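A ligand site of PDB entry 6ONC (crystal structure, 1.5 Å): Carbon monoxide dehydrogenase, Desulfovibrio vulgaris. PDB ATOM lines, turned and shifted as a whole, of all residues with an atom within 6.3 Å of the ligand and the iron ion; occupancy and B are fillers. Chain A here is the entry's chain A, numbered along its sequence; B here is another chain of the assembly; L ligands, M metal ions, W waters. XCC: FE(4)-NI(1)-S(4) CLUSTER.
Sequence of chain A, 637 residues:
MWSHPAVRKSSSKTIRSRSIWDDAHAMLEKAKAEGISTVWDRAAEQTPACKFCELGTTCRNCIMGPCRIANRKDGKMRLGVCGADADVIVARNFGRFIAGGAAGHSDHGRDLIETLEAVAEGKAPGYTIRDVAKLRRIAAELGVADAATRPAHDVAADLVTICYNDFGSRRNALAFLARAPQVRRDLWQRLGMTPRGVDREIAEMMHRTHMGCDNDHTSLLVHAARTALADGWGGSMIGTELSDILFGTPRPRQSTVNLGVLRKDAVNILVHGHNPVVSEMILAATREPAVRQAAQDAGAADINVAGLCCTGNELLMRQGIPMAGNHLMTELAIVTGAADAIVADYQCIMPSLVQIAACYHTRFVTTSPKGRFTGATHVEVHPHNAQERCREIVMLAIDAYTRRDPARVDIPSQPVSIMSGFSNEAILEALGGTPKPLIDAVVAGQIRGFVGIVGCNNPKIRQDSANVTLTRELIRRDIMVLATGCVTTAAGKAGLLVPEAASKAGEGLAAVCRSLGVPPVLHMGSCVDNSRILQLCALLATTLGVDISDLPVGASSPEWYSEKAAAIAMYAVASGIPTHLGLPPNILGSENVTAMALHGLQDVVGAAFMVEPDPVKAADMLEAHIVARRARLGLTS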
ATOM      1  N   HIS A 105      -9.833  10.993  14.443  1.00  0.00           N
ATOM      2  CA  HIS A 105     -10.285   9.622  14.211  1.00  0.00           C
ATOM      3  C   HIS A 105      -9.120   8.667  14.034  1.00  0.00           C
ATOM      4  O   HIS A 105      -9.220   7.494  14.403  1.00  0.00           O
ATOM      5  CB  HIS A 105     -11.218   9.595  13.006  1.00  0.00           C
ATOM      6  CG  HIS A 105     -12.525  10.283  13.262  1.00  0.00           C
ATOM      7  ND1 HIS A 105     -13.187  11.038  12.322  1.00  0.00           N
ATOM      8  CD2 HIS A 105     -13.299  10.324  14.382  1.00  0.00           C
ATOM      9  CE1 HIS A 105     -14.305  11.507  12.838  1.00  0.00           C
ATOM     10  NE2 HIS A 105     -14.393  11.084  14.087  1.00  0.00           N
ATOM     11  N   HIS A 272     -17.287  11.122  29.396  1.00  0.00           N
ATOM     12  CA  HIS A 272     -17.269  12.156  28.371  1.00  0.00           C
ATOM     13  C   HIS A 272     -16.068  11.925  27.478  1.00  0.00           C
ATOM     14  O   HIS A 272     -15.042  11.404  27.907  1.00  0.00           O
ATOM     15  CB  HIS A 272     -17.211  13.550  29.032  1.00  0.00           C
ATOM     16  CG  HIS A 272     -17.488  14.692  28.111  1.00  0.00           C
ATOM     17  ND1 HIS A 272     -17.901  14.525  26.806  1.00  0.00           N
ATOM     18  CD2 HIS A 272     -17.392  16.033  28.307  1.00  0.00           C
ATOM     19  CE1 HIS A 272     -18.047  15.703  26.238  1.00  0.00           C
ATOM     20  NE2 HIS A 272     -17.747  16.642  27.122  1.00  0.00           N
ATOM     21  N   GLY A 273     -16.216  12.289  26.211  1.00  0.00           N
ATOM     22  CA  GLY A 273     -15.142  12.036  25.261  1.00  0.00           C
ATOM     23  C   GLY A 273     -15.549  10.992  24.247  1.00  0.00           C
ATOM     24  O   GLY A 273     -16.696  11.029  23.765  1.00  0.00           O
ATOM     25  N   HIS A 274     -14.654  10.038  23.935  1.00  0.00           N
ATOM     26  CA  HIS A 274     -14.815   9.238  22.723  1.00  0.00           C
ATOM     27  C   HIS A 274     -14.587   7.738  22.802  1.00  0.00           C
ATOM     28  O   HIS A 274     -15.329   6.970  22.174  1.00  0.00           O
ATOM     29  CB  HIS A 274     -14.014   9.873  21.576  1.00  0.00           C
ATOM     30  CG  HIS A 274     -14.710  11.066  21.019  1.00  0.00           C
ATOM     31  ND1 HIS A 274     -14.687  12.279  21.661  1.00  0.00           N
ATOM     32  CD2 HIS A 274     -15.572  11.187  19.985  1.00  0.00           C
ATOM     33  CE1 HIS A 274     -15.484  13.122  21.009  1.00  0.00           C
ATOM     34  NE2 HIS A 274     -16.030  12.476  20.002  1.00  0.00           N
ATOM     35  N   CYS A 309     -21.918  12.675  24.830  1.00  0.00           N
ATOM     36  CA  CYS A 309     -21.209  12.736  23.549  1.00  0.00           C
ATOM     37  C   CYS A 309     -20.880  11.319  23.055  1.00  0.00           C
ATOM     38  O   CYS A 309     -21.648  10.375  23.317  1.00  0.00           O
ATOM     39  CB  CYS A 309     -20.064  13.700  23.661  1.00  0.00           C
ATOM     40  SG  CYS A 309     -20.637  15.415  23.837  1.00  0.00           S
ATOM     41  N   CYS A 310     -19.774  11.134  22.338  1.00  0.00           N
ATOM     42  CA  CYS A 310     -19.616   9.897  21.589  1.00  0.00           C
ATOM     43  C   CYS A 310     -19.338   8.703  22.490  1.00  0.00           C
ATOM     44  O   CYS A 310     -19.784   7.589  22.196  1.00  0.00           O
ATOM     45  CB  CYS A 310     -18.539  10.040  20.516  1.00  0.00           C
ATOM     46  SG  CYS A 310     -19.171  10.876  19.055  1.00  0.00           S
ATOM     47  N   THR A 311     -18.580   8.897  23.568  1.00  0.00           N
ATOM     48  CA  THR A 311     -18.399   7.765  24.452  1.00  0.00           C
ATOM     49  C   THR A 311     -19.733   7.359  25.080  1.00  0.00           C
ATOM     50  O   THR A 311     -19.988   6.175  25.307  1.00  0.00           O
ATOM     51  CB  THR A 311     -17.276   8.054  25.466  1.00  0.00           C
ATOM     52  OG1 THR A 311     -16.788   6.811  25.975  1.00  0.00           O
ATOM     53  CG2 THR A 311     -17.759   8.938  26.602  1.00  0.00           C
ATOM     54  N   ASN A 326     -25.889  15.739  24.753  1.00  0.00           N
ATOM     55  CA  ASN A 326     -24.948  15.982  23.665  1.00  0.00           C
ATOM     56  C   ASN A 326     -24.101  17.223  23.966  1.00  0.00           C
ATOM     57  O   ASN A 326     -24.141  17.779  25.063  1.00  0.00           O
ATOM     58  CB  ASN A 326     -25.690  16.002  22.318  1.00  0.00           C
ATOM     59  CG  ASN A 326     -26.914  16.906  22.325  1.00  0.00           C
ATOM     60  OD1 ASN A 326     -27.193  17.597  23.304  1.00  0.00           O
ATOM     61  ND2 ASN A 326     -27.666  16.894  21.210  1.00  0.00           N
ATOM     62  N   HIS A 327     -23.337  17.658  22.955  1.00  0.00           N
ATOM     63  CA  HIS A 327     -22.337  18.719  23.090  1.00  0.00           C
ATOM     64  C   HIS A 327     -22.759  19.906  23.954  1.00  0.00           C
ATOM     65  O   HIS A 327     -22.131  20.191  24.973  1.00  0.00           O
ATOM     66  CB  HIS A 327     -21.962  19.153  21.657  1.00  0.00           C
ATOM     67  CG  HIS A 327     -21.019  20.318  21.593  1.00  0.00           C
ATOM     68  ND1 HIS A 327     -20.012  20.534  22.506  1.00  0.00           N
ATOM     69  CD2 HIS A 327     -20.921  21.314  20.680  1.00  0.00           C
ATOM     70  CE1 HIS A 327     -19.342  21.621  22.173  1.00  0.00           C
ATOM     71  NE2 HIS A 327     -19.866  22.109  21.068  1.00  0.00           N
ATOM     72  N   GLN A 347     -11.238  14.706  22.940  1.00  0.00           N
ATOM     73  CA  GLN A 347     -12.026  15.312  21.867  1.00  0.00           C
ATOM     74  C   GLN A 347     -13.366  15.851  22.330  1.00  0.00           C
ATOM     75  O   GLN A 347     -14.153  15.124  22.944  1.00  0.00           O
ATOM     76  CB  GLN A 347     -12.253  14.360  20.686  1.00  0.00           C
ATOM     77  CG  GLN A 347     -10.984  13.867  20.048  1.00  0.00           C
ATOM     78  CD  GLN A 347     -11.229  12.685  19.154  1.00  0.00           C
ATOM     79  OE1 GLN A 347     -12.349  12.486  18.672  1.00  0.00           O
ATOM     80  NE2 GLN A 347     -10.186  11.887  18.940  1.00  0.00           N
ATOM     81  N   CYS A 348     -13.645  17.119  22.007  1.00  0.00           N
ATOM     82  CA  CYS A 348     -14.924  17.780  22.242  1.00  0.00           C
ATOM     83  C   CYS A 348     -15.207  18.025  23.710  1.00  0.00           C
ATOM     84  O   CYS A 348     -16.326  18.413  24.062  1.00  0.00           O
ATOM     85  CB  CYS A 348     -16.102  17.057  21.584  1.00  0.00           C
ATOM     86  SG  CYS A 348     -15.842  16.821  19.821  1.00  0.00           S
ATOM     87  N   VAL A 454     -25.994  13.489  11.182  1.00  0.00           N
ATOM     88  CA  VAL A 454     -24.763  13.210  11.915  1.00  0.00           C
ATOM     89  C   VAL A 454     -24.283  14.513  12.545  1.00  0.00           C
ATOM     90  O   VAL A 454     -24.787  15.601  12.253  1.00  0.00           O
ATOM     91  CB  VAL A 454     -23.692  12.615  10.970  1.00  0.00           C
ATOM     92  CG1 VAL A 454     -24.264  11.439  10.171  1.00  0.00           C
ATOM     93  CG2 VAL A 454     -23.179  13.677  10.019  1.00  0.00           C
ATOM     94  N   GLY A 455     -23.296  14.412  13.419  1.00  0.00           N
ATOM     95  CA  GLY A 455     -22.644  15.629  13.904  1.00  0.00           C
ATOM     96  C   GLY A 455     -23.320  16.313  15.073  1.00  0.00           C
ATOM     97  O   GLY A 455     -24.095  15.712  15.833  1.00  0.00           O
ATOM     98  N   CYS A 456     -23.055  17.617  15.187  1.00  0.00           N
ATOM     99  CA  CYS A 456     -22.860  18.316  16.455  1.00  0.00           C
ATOM    100  C   CYS A 456     -24.039  19.214  16.873  1.00  0.00           C
ATOM    101  O   CYS A 456     -25.168  19.106  16.370  1.00  0.00           O
ATOM    102  CB  CYS A 456     -21.583  19.174  16.339  1.00  0.00           C
ATOM    103  SG  CYS A 456     -20.146  18.432  15.438  1.00  0.00           S
ATOM    104  N   ASN A 457     -23.772  20.054  17.858  1.00  0.00           N
ATOM    105  CA  ASN A 457     -24.486  21.302  18.146  1.00  0.00           C
ATOM    106  C   ASN A 457     -23.521  22.449  17.887  1.00  0.00           C
ATOM    107  O   ASN A 457     -22.295  22.265  17.814  1.00  0.00           O
ATOM    108  CB  ASN A 457     -24.896  21.396  19.620  1.00  0.00           C
ATOM    109  CG  ASN A 457     -25.964  20.391  20.018  1.00  0.00           C
ATOM    110  OD1 ASN A 457     -26.833  20.004  19.226  1.00  0.00           O
ATOM    111  ND2 ASN A 457     -25.919  19.981  21.279  1.00  0.00           N
ATOM    112  N   THR A 484     -26.380   9.431  14.077  1.00  0.00           N
ATOM    113  CA  THR A 484     -25.138   9.180  14.809  1.00  0.00           C
ATOM    114  C   THR A 484     -24.738  10.433  15.576  1.00  0.00           C
ATOM    115  O   THR A 484     -25.249  11.529  15.330  1.00  0.00           O
ATOM    116  CB  THR A 484     -24.003   8.769  13.884  1.00  0.00           C
ATOM    117  OG1 THR A 484     -23.678   9.858  13.019  1.00  0.00           O
ATOM    118  CG2 THR A 484     -24.371   7.523  13.059  1.00  0.00           C
ATOM    119  N   GLY A 485     -23.809  10.247  16.504  1.00  0.00           N
ATOM    120  CA  GLY A 485     -23.186  11.377  17.180  1.00  0.00           C
ATOM    121  C   GLY A 485     -24.165  12.162  18.037  1.00  0.00           C
ATOM    122  O   GLY A 485     -25.081  11.603  18.646  1.00  0.00           O
ATOM    123  N   CYS A 486     -23.969  13.473  18.090  1.00  0.00           N
ATOM    124  CA  CYS A 486     -24.797  14.299  18.965  1.00  0.00           C
ATOM    125  C   CYS A 486     -26.235  14.431  18.474  1.00  0.00           C
ATOM    126  O   CYS A 486     -27.127  14.750  19.273  1.00  0.00           O
ATOM    127  CB  CYS A 486     -24.089  15.630  19.242  1.00  0.00           C
ATOM    128  SG  CYS A 486     -22.742  15.473  20.451  1.00  0.00           S
ATOM    129  N   VAL A 487     -26.498  14.167  17.198  1.00  0.00           N
ATOM    130  CA  VAL A 487     -27.869  14.079  16.710  1.00  0.00           C
ATOM    131  C   VAL A 487     -28.660  13.011  17.453  1.00  0.00           C
ATOM    132  O   VAL A 487     -29.887  13.145  17.631  1.00  0.00           O
ATOM    133  CB  VAL A 487     -27.868  13.832  15.187  1.00  0.00           C
ATOM    134  CG1 VAL A 487     -29.293  13.589  14.678  1.00  0.00           C
ATOM    135  CG2 VAL A 487     -27.202  14.985  14.462  1.00  0.00           C
ATOM    136  N   SER A 526     -21.733   6.187  17.345  1.00  0.00           N
ATOM    137  CA  SER A 526     -20.889   7.358  17.563  1.00  0.00           C
ATOM    138  C   SER A 526     -20.459   7.949  16.232  1.00  0.00           C
ATOM    139  O   SER A 526     -20.846   7.496  15.156  1.00  0.00           O
ATOM    140  CB  SER A 526     -19.654   6.928  18.318  1.00  0.00           C
ATOM    141  OG  SER A 526     -18.971   5.923  17.566  1.00  0.00           O
ATOM    142  N   CYS A 527     -19.612   8.981  16.293  1.00  0.00           N
ATOM    143  CA  CYS A 527     -19.124   9.617  15.065  1.00  0.00           C
ATOM    144  C   CYS A 527     -18.212   8.696  14.266  1.00  0.00           C
ATOM    145  O   CYS A 527     -18.212   8.760  13.022  1.00  0.00           O
ATOM    146  CB  CYS A 527     -18.399  10.918  15.400  1.00  0.00           C
ATOM    147  SG  CYS A 527     -19.512  12.273  15.737  1.00  0.00           S
ATOM    148  N   TYR A 561     -19.999  21.714  14.222  1.00  0.00           N
ATOM    149  CA  TYR A 561     -18.988  22.647  14.696  1.00  0.00           C
ATOM    150  C   TYR A 561     -17.545  22.176  14.457  1.00  0.00           C
ATOM    151  O   TYR A 561     -16.678  23.029  14.241  1.00  0.00           O
ATOM    152  CB  TYR A 561     -19.185  22.988  16.207  1.00  0.00           C
ATOM    153  CG  TYR A 561     -18.244  22.202  17.114  1.00  0.00           C
ATOM    154  CD1 TYR A 561     -16.961  22.666  17.347  1.00  0.00           C
ATOM    155  CD2 TYR A 561     -18.634  20.992  17.675  1.00  0.00           C
ATOM    156  CE1 TYR A 561     -16.069  21.943  18.096  1.00  0.00           C
ATOM    157  CE2 TYR A 561     -17.723  20.257  18.464  1.00  0.00           C
ATOM    158  CZ  TYR A 561     -16.444  20.753  18.654  1.00  0.00           C
ATOM    159  OH  TYR A 561     -15.512  20.064  19.388  1.00  0.00           O
ATOM    160  N   SER A 562     -17.248  20.873  14.509  1.00  0.00           N
ATOM    161  CA  SER A 562     -15.895  20.378  14.726  1.00  0.00           C
ATOM    162  C   SER A 562     -15.151  20.102  13.413  1.00  0.00           C
ATOM    163  O   SER A 562     -15.746  19.888  12.352  1.00  0.00           O
ATOM    164  CB  SER A 562     -15.931  19.085  15.537  1.00  0.00           C
ATOM    165  OG  SER A 562     -16.599  18.063  14.801  1.00  0.00           O
ATOM    166  N   LYS A 564     -13.700  17.314  13.043  1.00  0.00           N
ATOM    167  CA  LYS A 564     -14.120  15.946  12.767  1.00  0.00           C
ATOM    168  C   LYS A 564     -15.373  15.910  11.900  1.00  0.00           C
ATOM    169  O   LYS A 564     -15.485  15.077  10.990  1.00  0.00           O
ATOM    170  CB  LYS A 564     -14.364  15.186  14.079  1.00  0.00           C
ATOM    171  CG  LYS A 564     -13.096  14.645  14.711  1.00  0.00           C
ATOM    172  CD  LYS A 564     -13.413  13.960  16.037  1.00  0.00           C
ATOM    173  CE  LYS A 564     -13.940  14.960  17.043  1.00  0.00           C
ATOM    174  NZ  LYS A 564     -14.541  14.190  18.192  1.00  0.00           N
ATOM    175  N   ALA A 565     -16.330  16.802  12.170  1.00  0.00           N
ATOM    176  CA  ALA A 565     -17.566  16.819  11.388  1.00  0.00           C
ATOM    177  C   ALA A 565     -17.275  17.217   9.943  1.00  0.00           C
ATOM    178  O   ALA A 565     -17.885  16.670   9.007  1.00  0.00           O
ATOM    179  CB  ALA A 565     -18.583  17.758  12.021  1.00  0.00           C
ATOM    180  N   ILE A 568     -15.873  14.108   8.246  1.00  0.00           N
ATOM    181  CA  ILE A 568     -16.970  13.189   7.917  1.00  0.00           C
ATOM    182  C   ILE A 568     -17.729  13.648   6.676  1.00  0.00           C
ATOM    183  O   ILE A 568     -17.992  12.859   5.761  1.00  0.00           O
ATOM    184  CB  ILE A 568     -17.898  13.021   9.131  1.00  0.00           C
ATOM    185  CG1 ILE A 568     -17.192  12.259  10.264  1.00  0.00           C
ATOM    186  CG2 ILE A 568     -19.205  12.307   8.729  1.00  0.00           C
ATOM    187  CD1 ILE A 568     -17.789  12.512  11.624  1.00  0.00           C
ATOM    188  N   HIS B 210      -7.046  19.560  18.085  1.00  0.00           N
ATOM    189  CA  HIS B 210      -8.489  19.632  17.857  1.00  0.00           C
ATOM    190  C   HIS B 210      -9.165  20.145  19.122  1.00  0.00           C
ATOM    191  O   HIS B 210      -8.659  19.940  20.239  1.00  0.00           O
ATOM    192  CB  HIS B 210      -9.010  18.220  17.530  1.00  0.00           C
ATOM    193  CG  HIS B 210     -10.446  18.164  17.110  1.00  0.00           C
ATOM    194  ND1 HIS B 210     -11.508  18.259  17.993  1.00  0.00           N
ATOM    195  CD2 HIS B 210     -11.003  17.977  15.887  1.00  0.00           C
ATOM    196  CE1 HIS B 210     -12.652  18.141  17.328  1.00  0.00           C
ATOM    197  NE2 HIS B 210     -12.366  17.984  16.047  1.00  0.00           N
HETATM  198 FE1  XCC L   1     -18.033  16.169  19.004  1.00  0.00          FE
HETATM  199 FE2  XCC L   1     -17.902  12.838  18.901  1.00  0.00          FE
HETATM  200 FE3  XCC L   1     -19.635  16.645  17.031  1.00  0.00          FE
HETATM  201 FE4  XCC L   1     -20.693  15.564  19.216  1.00  0.00          FE
HETATM  202  S1  XCC L   1     -21.075  14.925  17.083  1.00  0.00           S
HETATM  203  S2  XCC L   1     -19.794  17.586  19.092  1.00  0.00           S
HETATM  204  S4  XCC L   1     -17.552  15.944  16.855  1.00  0.00           S
HETATM  205  S3  XCC L   1     -18.908  14.443  20.167  1.00  0.00           S
HETATM  206 FE    FE M   1     -19.045  13.949  17.564  1.00  0.00          FE
HETATM  207  O   HOH W   1     -16.819  12.955  17.333  1.00  0.00           O
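A ring nitrogen (NE2) of His 274 binds an iron atom (FE2) of the ligand (2.2 Å). SG of Cys 310 binds FE2 of the ligand (2.3 Å). N of Cys 486 sits close to S1 of the ligand. SG of Cys 486 binds FE4 of the ligand, 2.4 Å away. The side-chain sulfur (SG) of Cys 348 is bound to an iron atom (FE1) of the ligand. SG of Cys 456 is bound to FE3 of the ligand, 2.4 Å away. A sulfur (S4) of the ligand sits close to the side-chain hydroxyl (OG) of Ser 562 (3.1 Å). A sulfur (S4) of the ligand sits close to the side-chain amino group of Lys 564, at 3.7 Å.
ND1 of His 274 sits close to O of Gln 347, at 3.2 Å. The backbone NH (N) of Cys 310 lies within hydrogen-bond range of the backbone carbonyl oxygen (O) of Gly 273 (3.4 Å). N of Cys 486 sits at hydrogen-bond distance from O of Gly 455 (3.2 Å). The backbone NH of His 327 sits close to the side-chain sulfur of Cys 486 (3.4 Å). SG of Cys 348 sits close to OH of Tyr 561, 3.3 Å away. OG of Ser 562 sits close to SG of Cys 456 (3.6 Å). The backbone NH (N) of Tyr 561 sits close to the side-chain sulfur (SG) of Cys 456 (3.5 Å). The backbone carbonyl oxygen of Gly 455 sits at hydrogen-bond distance from the backbone NH of Val 487 (3.2 Å).
Cys 310 touches the iron ion. Within 4 Å of the iron ion: Cys 310 and Cys 527. Along chain A the residues within 4 Å of the iron ion span positions 310 to 527. The nearest printed residue that does not touch the iron ion is His 274 (4.1 Å).
S1 of the ligand sits close to O of Gly 455 (3.4 Å). Merely in contact with the ligand: Tyr 561 (3.4 Å), His 327 (3.7 Å) and Cys 309 (3.8 Å). Hydrophobic or aromatic side chains within 4 Å of the ligand: His 274, His 327 and Tyr 561. Of the 27 residues printed, 12 come within 4 Å of the ligand. Along chain A the residues within 4 Å of the ligand span positions 274 to 564. The nearest printed residue that does not touch the ligand is Gly 485 (4.1 Å).
S1 of the ligand is bound to the iron ion, at 2.3 Å. The iron ion is bound by water W1, 2.4 Å away. The side-chain sulfur (SG) of Cys 527 is bound to the iron ion (2.5 Å). The iron ion is bound by S4 of the ligand (2.6 Å). The iron ion is bound by a sulfur (S3) of the ligand (2.7 Å). The iron ion has five donor atoms within binding distance.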
